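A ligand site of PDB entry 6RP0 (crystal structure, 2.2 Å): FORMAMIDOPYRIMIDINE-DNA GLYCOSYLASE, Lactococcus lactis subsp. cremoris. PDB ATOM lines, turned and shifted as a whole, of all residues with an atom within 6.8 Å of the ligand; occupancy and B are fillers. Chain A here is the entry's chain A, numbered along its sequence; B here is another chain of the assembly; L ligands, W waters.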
ATOM      1  N   LYS A  57      -6.228 -16.217  26.600  1.00  0.00           N
ATOM      2  CA  LYS A  57      -6.919 -15.303  27.502  1.00  0.00           C
ATOM      3  C   LYS A  57      -8.399 -15.633  27.680  1.00  0.00           C
ATOM      4  O   LYS A  57      -9.126 -14.893  28.325  1.00  0.00           O
ATOM      5  CB  LYS A  57      -6.789 -13.863  26.992  1.00  0.00           C
ATOM      6  CG  LYS A  57      -5.341 -13.425  26.718  1.00  0.00           C
ATOM      7  CD  LYS A  57      -5.265 -12.001  26.186  1.00  0.00           C
ATOM      8  CE  LYS A  57      -3.850 -11.692  25.722  1.00  0.00           C
ATOM      9  NZ  LYS A  57      -3.755 -10.453  24.890  1.00  0.00           N
ATOM     10  N   TYR A  58      -8.849 -16.755  27.088  1.00  0.00           N
ATOM     11  CA  TYR A  58     -10.263 -17.132  27.165  1.00  0.00           C
ATOM     12  C   TYR A  58     -10.554 -18.071  28.321  1.00  0.00           C
ATOM     13  O   TYR A  58      -9.904 -19.110  28.453  1.00  0.00           O
ATOM     14  CB  TYR A  58     -10.703 -17.834  25.883  1.00  0.00           C
ATOM     15  CG  TYR A  58     -10.718 -17.006  24.636  1.00  0.00           C
ATOM     16  CD1 TYR A  58      -9.528 -16.675  23.983  1.00  0.00           C
ATOM     17  CD2 TYR A  58     -11.918 -16.595  24.060  1.00  0.00           C
ATOM     18  CE1 TYR A  58      -9.545 -15.943  22.798  1.00  0.00           C
ATOM     19  CE2 TYR A  58     -11.942 -15.863  22.888  1.00  0.00           C
ATOM     20  CZ  TYR A  58     -10.751 -15.536  22.259  1.00  0.00           C
ATOM     21  OH  TYR A  58     -10.788 -14.798  21.103  1.00  0.00           O
ATOM     22  N   ILE A 131      -5.623 -19.224  17.282  1.00  0.00           N
ATOM     23  CA  ILE A 131      -4.873 -19.110  18.539  1.00  0.00           C
ATOM     24  C   ILE A 131      -3.664 -20.038  18.553  1.00  0.00           C
ATOM     25  O   ILE A 131      -3.778 -21.226  18.276  1.00  0.00           O
ATOM     26  CB  ILE A 131      -5.775 -19.424  19.764  1.00  0.00           C
ATOM     27  CG1 ILE A 131      -6.965 -18.481  19.793  1.00  0.00           C
ATOM     28  CG2 ILE A 131      -5.010 -19.275  21.054  1.00  0.00           C
ATOM     29  CD1 ILE A 131      -6.594 -17.027  19.724  1.00  0.00           C
ATOM     30  N   PRO A 158       4.005  -6.200  17.836  1.00  0.00           N
ATOM     31  CA  PRO A 158       2.630  -6.477  17.386  1.00  0.00           C
ATOM     32  C   PRO A 158       2.404  -7.904  16.889  1.00  0.00           C
ATOM     33  O   PRO A 158       1.273  -8.384  16.942  1.00  0.00           O
ATOM     34  CB  PRO A 158       2.407  -5.483  16.245  1.00  0.00           C
ATOM     35  CG  PRO A 158       3.772  -5.100  15.787  1.00  0.00           C
ATOM     36  CD  PRO A 158       4.658  -5.163  17.011  1.00  0.00           C
ATOM     37  N   LEU A 160       3.773 -10.729  18.237  1.00  0.00           N
ATOM     38  CA  LEU A 160       3.536 -11.481  19.474  1.00  0.00           C
ATOM     39  C   LEU A 160       2.114 -11.286  20.000  1.00  0.00           C
ATOM     40  O   LEU A 160       1.464 -12.238  20.441  1.00  0.00           O
ATOM     41  CB  LEU A 160       4.570 -11.098  20.554  1.00  0.00           C
ATOM     42  CG  LEU A 160       5.992 -11.645  20.361  1.00  0.00           C
ATOM     43  CD1 LEU A 160       6.963 -11.099  21.376  1.00  0.00           C
ATOM     44  CD2 LEU A 160       6.001 -13.179  20.413  1.00  0.00           C
ATOM     45  N   LEU A 161       1.612 -10.053  19.929  1.00  0.00           N
ATOM     46  CA  LEU A 161       0.288  -9.720  20.431  1.00  0.00           C
ATOM     47  C   LEU A 161      -0.845 -10.316  19.592  1.00  0.00           C
ATOM     48  O   LEU A 161      -1.996 -10.336  20.030  1.00  0.00           O
ATOM     49  CB  LEU A 161       0.116  -8.193  20.500  1.00  0.00           C
ATOM     50  CG  LEU A 161       0.938  -7.459  21.581  1.00  0.00           C
ATOM     51  CD1 LEU A 161       0.750  -5.946  21.471  1.00  0.00           C
ATOM     52  CD2 LEU A 161       0.601  -7.941  22.995  1.00  0.00           C
ATOM     53  N   GLU A 162      -0.522 -10.814  18.389  1.00  0.00           N
ATOM     54  CA  GLU A 162      -1.559 -11.389  17.515  1.00  0.00           C
ATOM     55  C   GLU A 162      -2.178 -12.683  18.071  1.00  0.00           C
ATOM     56  O   GLU A 162      -3.193 -13.138  17.567  1.00  0.00           O
ATOM     57  CB  GLU A 162      -1.003 -11.701  16.119  1.00  0.00           C
ATOM     58  CG  GLU A 162      -0.817 -10.501  15.224  1.00  0.00           C
ATOM     59  CD  GLU A 162      -0.410 -10.904  13.794  1.00  0.00           C
ATOM     60  OE1 GLU A 162      -0.386 -12.116  13.488  1.00  0.00           O
ATOM     61  OE2 GLU A 162      -0.106  -9.995  12.992  1.00  0.00           O
ATOM     62  N   GLN A 163      -1.524 -13.265  19.077  1.00  0.00           N
ATOM     63  CA  GLN A 163      -1.958 -14.514  19.729  1.00  0.00           C
ATOM     64  C   GLN A 163      -1.691 -15.756  18.861  1.00  0.00           C
ATOM     65  O   GLN A 163      -2.090 -16.852  19.236  1.00  0.00           O
ATOM     66  CB  GLN A 163      -3.452 -14.473  20.091  1.00  0.00           C
ATOM     67  CG  GLN A 163      -3.880 -13.321  20.990  1.00  0.00           C
ATOM     68  CD  GLN A 163      -3.002 -13.204  22.213  1.00  0.00           C
ATOM     69  OE1 GLN A 163      -3.024 -14.083  23.083  1.00  0.00           O
ATOM     70  NE2 GLN A 163      -2.209 -12.122  22.290  1.00  0.00           N
ATOM     71  N   LEU A 169      -0.074 -13.477  25.606  1.00  0.00           N
ATOM     72  CA  LEU A 169       0.622 -12.228  25.875  1.00  0.00           C
ATOM     73  C   LEU A 169      -0.278 -11.034  25.575  1.00  0.00           C
ATOM     74  O   LEU A 169      -0.968 -11.001  24.556  1.00  0.00           O
ATOM     75  CB  LEU A 169       1.905 -12.124  25.043  1.00  0.00           C
ATOM     76  CG  LEU A 169       3.054 -13.077  25.339  1.00  0.00           C
ATOM     77  CD1 LEU A 169       4.018 -13.070  24.143  1.00  0.00           C
ATOM     78  CD2 LEU A 169       3.787 -12.685  26.640  1.00  0.00           C
ATOM     79  N   GLY A 170      -0.295 -10.068  26.488  1.00  0.00           N
ATOM     80  CA  GLY A 170      -0.952  -8.797  26.267  1.00  0.00           C
ATOM     81  C   GLY A 170       0.083  -7.679  26.479  1.00  0.00           C
ATOM     82  O   GLY A 170       1.270  -7.964  26.557  1.00  0.00           O
ATOM     83  N   ASN A 171      -0.366  -6.427  26.583  1.00  0.00           N
ATOM     84  CA  ASN A 171       0.555  -5.293  26.523  1.00  0.00           C
ATOM     85  C   ASN A 171       1.568  -5.288  27.664  1.00  0.00           C
ATOM     86  O   ASN A 171       2.731  -4.948  27.449  1.00  0.00           O
ATOM     87  CB  ASN A 171      -0.207  -3.968  26.511  1.00  0.00           C
ATOM     88  CG  ASN A 171       0.562  -2.838  25.800  1.00  0.00           C
ATOM     89  OD1 ASN A 171       1.235  -3.059  24.803  1.00  0.00           O
ATOM     90  ND2 ASN A 171       0.437  -1.622  26.326  1.00  0.00           N
ATOM     91  N   ARG A 260      -0.176   0.652  20.361  1.00  0.00           N
ATOM     92  CA  ARG A 260      -0.113   0.331  21.788  1.00  0.00           C
ATOM     93  C   ARG A 260       0.988   1.118  22.483  1.00  0.00           C
ATOM     94  O   ARG A 260       2.073   1.338  21.932  1.00  0.00           O
ATOM     95  CB  ARG A 260       0.124  -1.168  21.999  1.00  0.00           C
ATOM     96  CG  ARG A 260      -0.840  -2.086  21.232  1.00  0.00           C
ATOM     97  CD  ARG A 260      -2.294  -1.816  21.644  1.00  0.00           C
ATOM     98  NE  ARG A 260      -2.549  -2.031  23.067  1.00  0.00           N
ATOM     99  CZ  ARG A 260      -2.867  -3.219  23.615  1.00  0.00           C
ATOM    100  NH1 ARG A 260      -2.964  -4.313  22.855  1.00  0.00           N
ATOM    101  NH2 ARG A 260      -3.100  -3.304  24.915  1.00  0.00           N
ATOM    102  O5' 3DR B   7      -3.364  -2.632  28.182  1.00  0.00           O
ATOM    103  P   3DR B   7      -2.912  -1.146  27.965  1.00  0.00           P
ATOM    104  OP1 3DR B   7      -1.443  -0.960  28.320  1.00  0.00           O
ATOM    105  OP2 3DR B   7      -3.182  -0.740  26.529  1.00  0.00           O
ATOM    106  C2' 3DR B   7      -5.499  -5.317  29.606  1.00  0.00           C
ATOM    107  C5' 3DR B   7      -3.235  -3.276  29.382  1.00  0.00           C
ATOM    108  C4' 3DR B   7      -3.317  -4.778  29.327  1.00  0.00           C
ATOM    109  O4' 3DR B   7      -3.387  -5.309  30.613  1.00  0.00           O
ATOM    110  C1' 3DR B   7      -4.720  -5.669  30.839  1.00  0.00           C
ATOM    111  C3' 3DR B   7      -4.538  -5.253  28.611  1.00  0.00           C
ATOM    112  O3' 3DR B   7      -4.334  -6.558  28.193  1.00  0.00           O
ATOM    113  P    DT B   8      -4.270  -6.923  26.638  1.00  0.00           P
ATOM    114  OP1  DT B   8      -3.967  -8.365  26.530  1.00  0.00           O
ATOM    115  OP2  DT B   8      -3.392  -5.942  25.944  1.00  0.00           O
ATOM    116  O5'  DT B   8      -5.775  -6.685  26.133  1.00  0.00           O
ATOM    117  C5'  DT B   8      -6.817  -7.423  26.723  1.00  0.00           C
ATOM    118  C4'  DT B   8      -7.729  -8.031  25.675  1.00  0.00           C
ATOM    119  O4'  DT B   8      -8.595  -7.001  25.165  1.00  0.00           O
ATOM    120  C3'  DT B   8      -7.037  -8.669  24.480  1.00  0.00           C
ATOM    121  O3'  DT B   8      -7.595  -9.966  24.270  1.00  0.00           O
ATOM    122  C2'  DT B   8      -7.303  -7.705  23.306  1.00  0.00           C
ATOM    123  C1'  DT B   8      -8.534  -6.928  23.762  1.00  0.00           C
ATOM    124  N1   DT B   8      -8.573  -5.460  23.402  1.00  0.00           N
ATOM    125  C2   DT B   8      -9.741  -4.934  22.894  1.00  0.00           C
ATOM    126  O2   DT B   8     -10.729  -5.592  22.684  1.00  0.00           O
ATOM    127  N3   DT B   8      -9.702  -3.596  22.632  1.00  0.00           N
ATOM    128  C4   DT B   8      -8.640  -2.741  22.813  1.00  0.00           C
ATOM    129  O4   DT B   8      -8.724  -1.549  22.537  1.00  0.00           O
ATOM    130  C5   DT B   8      -7.447  -3.333  23.374  1.00  0.00           C
ATOM    131  C7   DT B   8      -6.231  -2.471  23.626  1.00  0.00           C
ATOM    132  C6   DT B   8      -7.468  -4.653  23.655  1.00  0.00           C
ATOM    133  P    DT B   9      -7.104 -10.934  23.086  1.00  0.00           P
ATOM    134  OP1  DT B   9      -7.444 -12.297  23.553  1.00  0.00           O
ATOM    135  OP2  DT B   9      -5.699 -10.592  22.746  1.00  0.00           O
ATOM    136  O5'  DT B   9      -8.060 -10.567  21.869  1.00  0.00           O
ATOM    137  C5'  DT B   9      -9.441 -10.829  22.014  1.00  0.00           C
ATOM    138  C4'  DT B   9     -10.254 -10.131  20.953  1.00  0.00           C
ATOM    139  O4'  DT B   9     -10.036  -8.703  21.002  1.00  0.00           O
ATOM    140  C3'  DT B   9      -9.964 -10.576  19.523  1.00  0.00           C
ATOM    141  O3'  DT B   9     -11.113 -11.206  19.070  1.00  0.00           O
ATOM    142  C2'  DT B   9      -9.691  -9.251  18.767  1.00  0.00           C
ATOM    143  C1'  DT B   9     -10.266  -8.195  19.719  1.00  0.00           C
ATOM    144  N1   DT B   9      -9.622  -6.856  19.654  1.00  0.00           N
ATOM    145  C2   DT B   9     -10.390  -5.764  19.337  1.00  0.00           C
ATOM    146  O2   DT B   9     -11.565  -5.827  19.082  1.00  0.00           O
ATOM    147  N3   DT B   9      -9.724  -4.581  19.338  1.00  0.00           N
ATOM    148  C4   DT B   9      -8.390  -4.374  19.610  1.00  0.00           C
ATOM    149  O4   DT B   9      -7.877  -3.268  19.573  1.00  0.00           O
ATOM    150  C5   DT B   9      -7.635  -5.573  19.951  1.00  0.00           C
ATOM    151  C7   DT B   9      -6.170  -5.478  20.278  1.00  0.00           C
ATOM    152  C6   DT B   9      -8.283  -6.739  19.968  1.00  0.00           C
ATOM    153  P    DT B  10     -11.209 -11.891  17.623  1.00  0.00           P
ATOM    154  OP1  DT B  10     -12.274 -12.900  17.817  1.00  0.00           O
ATOM    155  OP2  DT B  10      -9.868 -12.243  17.106  1.00  0.00           O
ATOM    156  O5'  DT B  10     -11.787 -10.717  16.701  1.00  0.00           O
ATOM    157  C5'  DT B  10     -12.977 -10.083  17.048  1.00  0.00           C
ATOM    158  C4'  DT B  10     -13.266  -8.941  16.100  1.00  0.00           C
ATOM    159  O4'  DT B  10     -12.452  -7.795  16.440  1.00  0.00           O
ATOM    160  C3'  DT B  10     -13.002  -9.256  14.632  1.00  0.00           C
ATOM    161  O3'  DT B  10     -14.202  -9.117  13.906  1.00  0.00           O
ATOM    162  C2'  DT B  10     -11.958  -8.206  14.201  1.00  0.00           C
ATOM    163  C1'  DT B  10     -12.099  -7.127  15.265  1.00  0.00           C
ATOM    164  N1   DT B  10     -10.851  -6.404  15.531  1.00  0.00           N
ATOM    165  C2   DT B  10     -10.843  -5.036  15.454  1.00  0.00           C
ATOM    166  O2   DT B  10     -11.827  -4.377  15.147  1.00  0.00           O
ATOM    167  N3   DT B  10      -9.638  -4.455  15.735  1.00  0.00           N
ATOM    168  C4   DT B  10      -8.462  -5.099  16.083  1.00  0.00           C
ATOM    169  O4   DT B  10      -7.419  -4.491  16.323  1.00  0.00           O
ATOM    170  C5   DT B  10      -8.543  -6.540  16.151  1.00  0.00           C
ATOM    171  C7   DT B  10      -7.332  -7.336  16.516  1.00  0.00           C
ATOM    172  C6   DT B  10      -9.719  -7.117  15.879  1.00  0.00           C
ATOM    173  P    DC B  11     -14.284  -9.524  12.359  1.00  0.00           P
ATOM    174  OP1  DC B  11     -15.562 -10.238  12.205  1.00  0.00           O
ATOM    175  OP2  DC B  11     -13.030 -10.141  11.862  1.00  0.00           O
ATOM    176  O5'  DC B  11     -14.381  -8.106  11.634  1.00  0.00           O
ATOM    177  C5'  DC B  11     -15.290  -7.131  12.126  1.00  0.00           C
ATOM    178  C4'  DC B  11     -14.984  -5.804  11.485  1.00  0.00           C
ATOM    179  O4'  DC B  11     -13.818  -5.258  12.108  1.00  0.00           O
ATOM    180  C3'  DC B  11     -14.693  -5.865   9.981  1.00  0.00           C
ATOM    181  O3'  DC B  11     -15.695  -5.159   9.252  1.00  0.00           O
ATOM    182  C2'  DC B  11     -13.316  -5.219   9.816  1.00  0.00           C
ATOM    183  C1'  DC B  11     -13.060  -4.555  11.173  1.00  0.00           C
ATOM    184  N1   DC B  11     -11.640  -4.627  11.585  1.00  0.00           N
ATOM    185  C2   DC B  11     -10.900  -3.459  11.732  1.00  0.00           C
ATOM    186  O2   DC B  11     -11.456  -2.364  11.516  1.00  0.00           O
ATOM    187  N3   DC B  11      -9.595  -3.554  12.080  1.00  0.00           N
ATOM    188  C4   DC B  11      -9.038  -4.749  12.287  1.00  0.00           C
ATOM    189  N4   DC B  11      -7.754  -4.805  12.641  1.00  0.00           N
ATOM    190  C5   DC B  11      -9.779  -5.957  12.131  1.00  0.00           C
ATOM    191  C6   DC B  11     -11.067  -5.849  11.784  1.00  0.00           C
HETATM  192  C1  LIG L   1      -3.801  -7.996  19.064  1.00  0.00           C
HETATM  193  C2  LIG L   1      -4.646  -9.014  19.444  1.00  0.00           C
HETATM  194  C3  LIG L   1      -5.241  -9.784  18.471  1.00  0.00           C
HETATM  195  C4  LIG L   1      -3.880  -8.045  21.137  1.00  0.00           C
HETATM  196  N1  LIG L   1      -4.967  -9.494  17.173  1.00  0.00           N
HETATM  197  N2  LIG L   1      -3.530  -7.719  17.780  1.00  0.00           N
HETATM  198  O1  LIG L   1      -6.003 -10.709  18.826  1.00  0.00           O
HETATM  199  N3  LIG L   1      -4.695  -9.047  20.790  1.00  0.00           N
HETATM  200  S1  LIG L   1      -3.586  -7.680  22.825  1.00  0.00           S
HETATM  201  N4  LIG L   1      -3.300  -7.349  20.128  1.00  0.00           N
HETATM  202  C5  LIG L   1      -4.129  -8.479  16.829  1.00  0.00           C
HETATM  203  S2  LIG L   1      -3.789  -8.122  15.181  1.00  0.00           S
HETATM  204  O   HOH W   1      -0.948  -6.748  16.986  1.00  0.00           O
HETATM  205  O   HOH W   2      -2.483  -4.829  19.977  1.00  0.00           O
HETATM  206  O   HOH W   3      -4.510  -5.218  15.939  1.00  0.00           O
HETATM  207  O   HOH W   4      -6.193  -7.338  12.814  1.00  0.00           O
HETATM  208  O   HOH W   5      -5.019 -12.346  15.616  1.00  0.00           O
HETATM  209  O   HOH W   6      -7.038 -13.219  18.873  1.00  0.00           O
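Water W2 lies within hydrogen-bond range of a nitrogen (N4) of the ligand and the guanidinium group (NH1) of Arg 260.
Water W6 lies within hydrogen-bond range of an oxygen (O1) of the ligand (2.7 Å) and OP2 of DT 10 of chain B (3.5 Å).
Water W1 lies within hydrogen-bond range of the backbone carbonyl oxygen of Pro 158 (2.8 Å) and a nitrogen (N2) of the ligand (2.9 Å).
Water W3 bridges O4 of DT 10 of chain B (3.0 Å) and a sulfur (S2) of the ligand (3.1 Å).
Water W5 bridges O of Glu 162 (2.8 Å) and N1 of the ligand (3.2 Å).
Water W4 lies within hydrogen-bond range of N4 of DC 11 of chain B (3.0 Å) and a sulfur (S2) of the ligand (3.5 Å).
NH2 of Arg 260 lies within salt-bridge range of OP2 of DT 8 of chain B (2.8 Å).
O of Leu 161 lies within hydrogen-bond range of NE2 of Gln 163 (2.9 Å).
OP2 of 3DR 7 of chain B lies within salt-bridge range of the guanidinium group (NH2) of Arg 260 (3.0 Å).
NZ of Lys 57 is in salt-bridge range of OP2 of DT 9 of chain B (2.9 Å).
NZ of Lys 57 lies within hydrogen-bond range of O of Leu 169 (2.9 Å).
NZ of Lys 57 lies close to NE2 of Gln 163 (3.5 Å).
The side-chain amino group (NZ) of Lys 57 is in salt-bridge range of OP1 of DT 8 of chain B, 2.7 Å away.
OP2 of DT 8 of chain B lies within hydrogen-bond range of N of Asn 171 (3.1 Å).
S1 of the ligand lies close to OP2 of DT 8 of chain B (3.6 Å).
Glu 162 touches the ligand (CG to S2, 3.8 Å).
DT 10 of chain B touches the ligand.
The nearest printed residue that does not touch the ligand is Gln 163 (4.002 Å).
The backbone carbonyl oxygen (O) of Leu 161 sits close to a nitrogen (N3) of the ligand, 3.1 Å away.
NH1 of Arg 260 sits close to S1 of the ligand (3.4 Å).
A nitrogen (N3) of the ligand lies within hydrogen-bond range of OP2 of DT 9 of chain B, at 2.7 Å.
A sulfur (S1) of the ligand lies close to the side-chain amino group of Lys 57 (3.5 Å).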
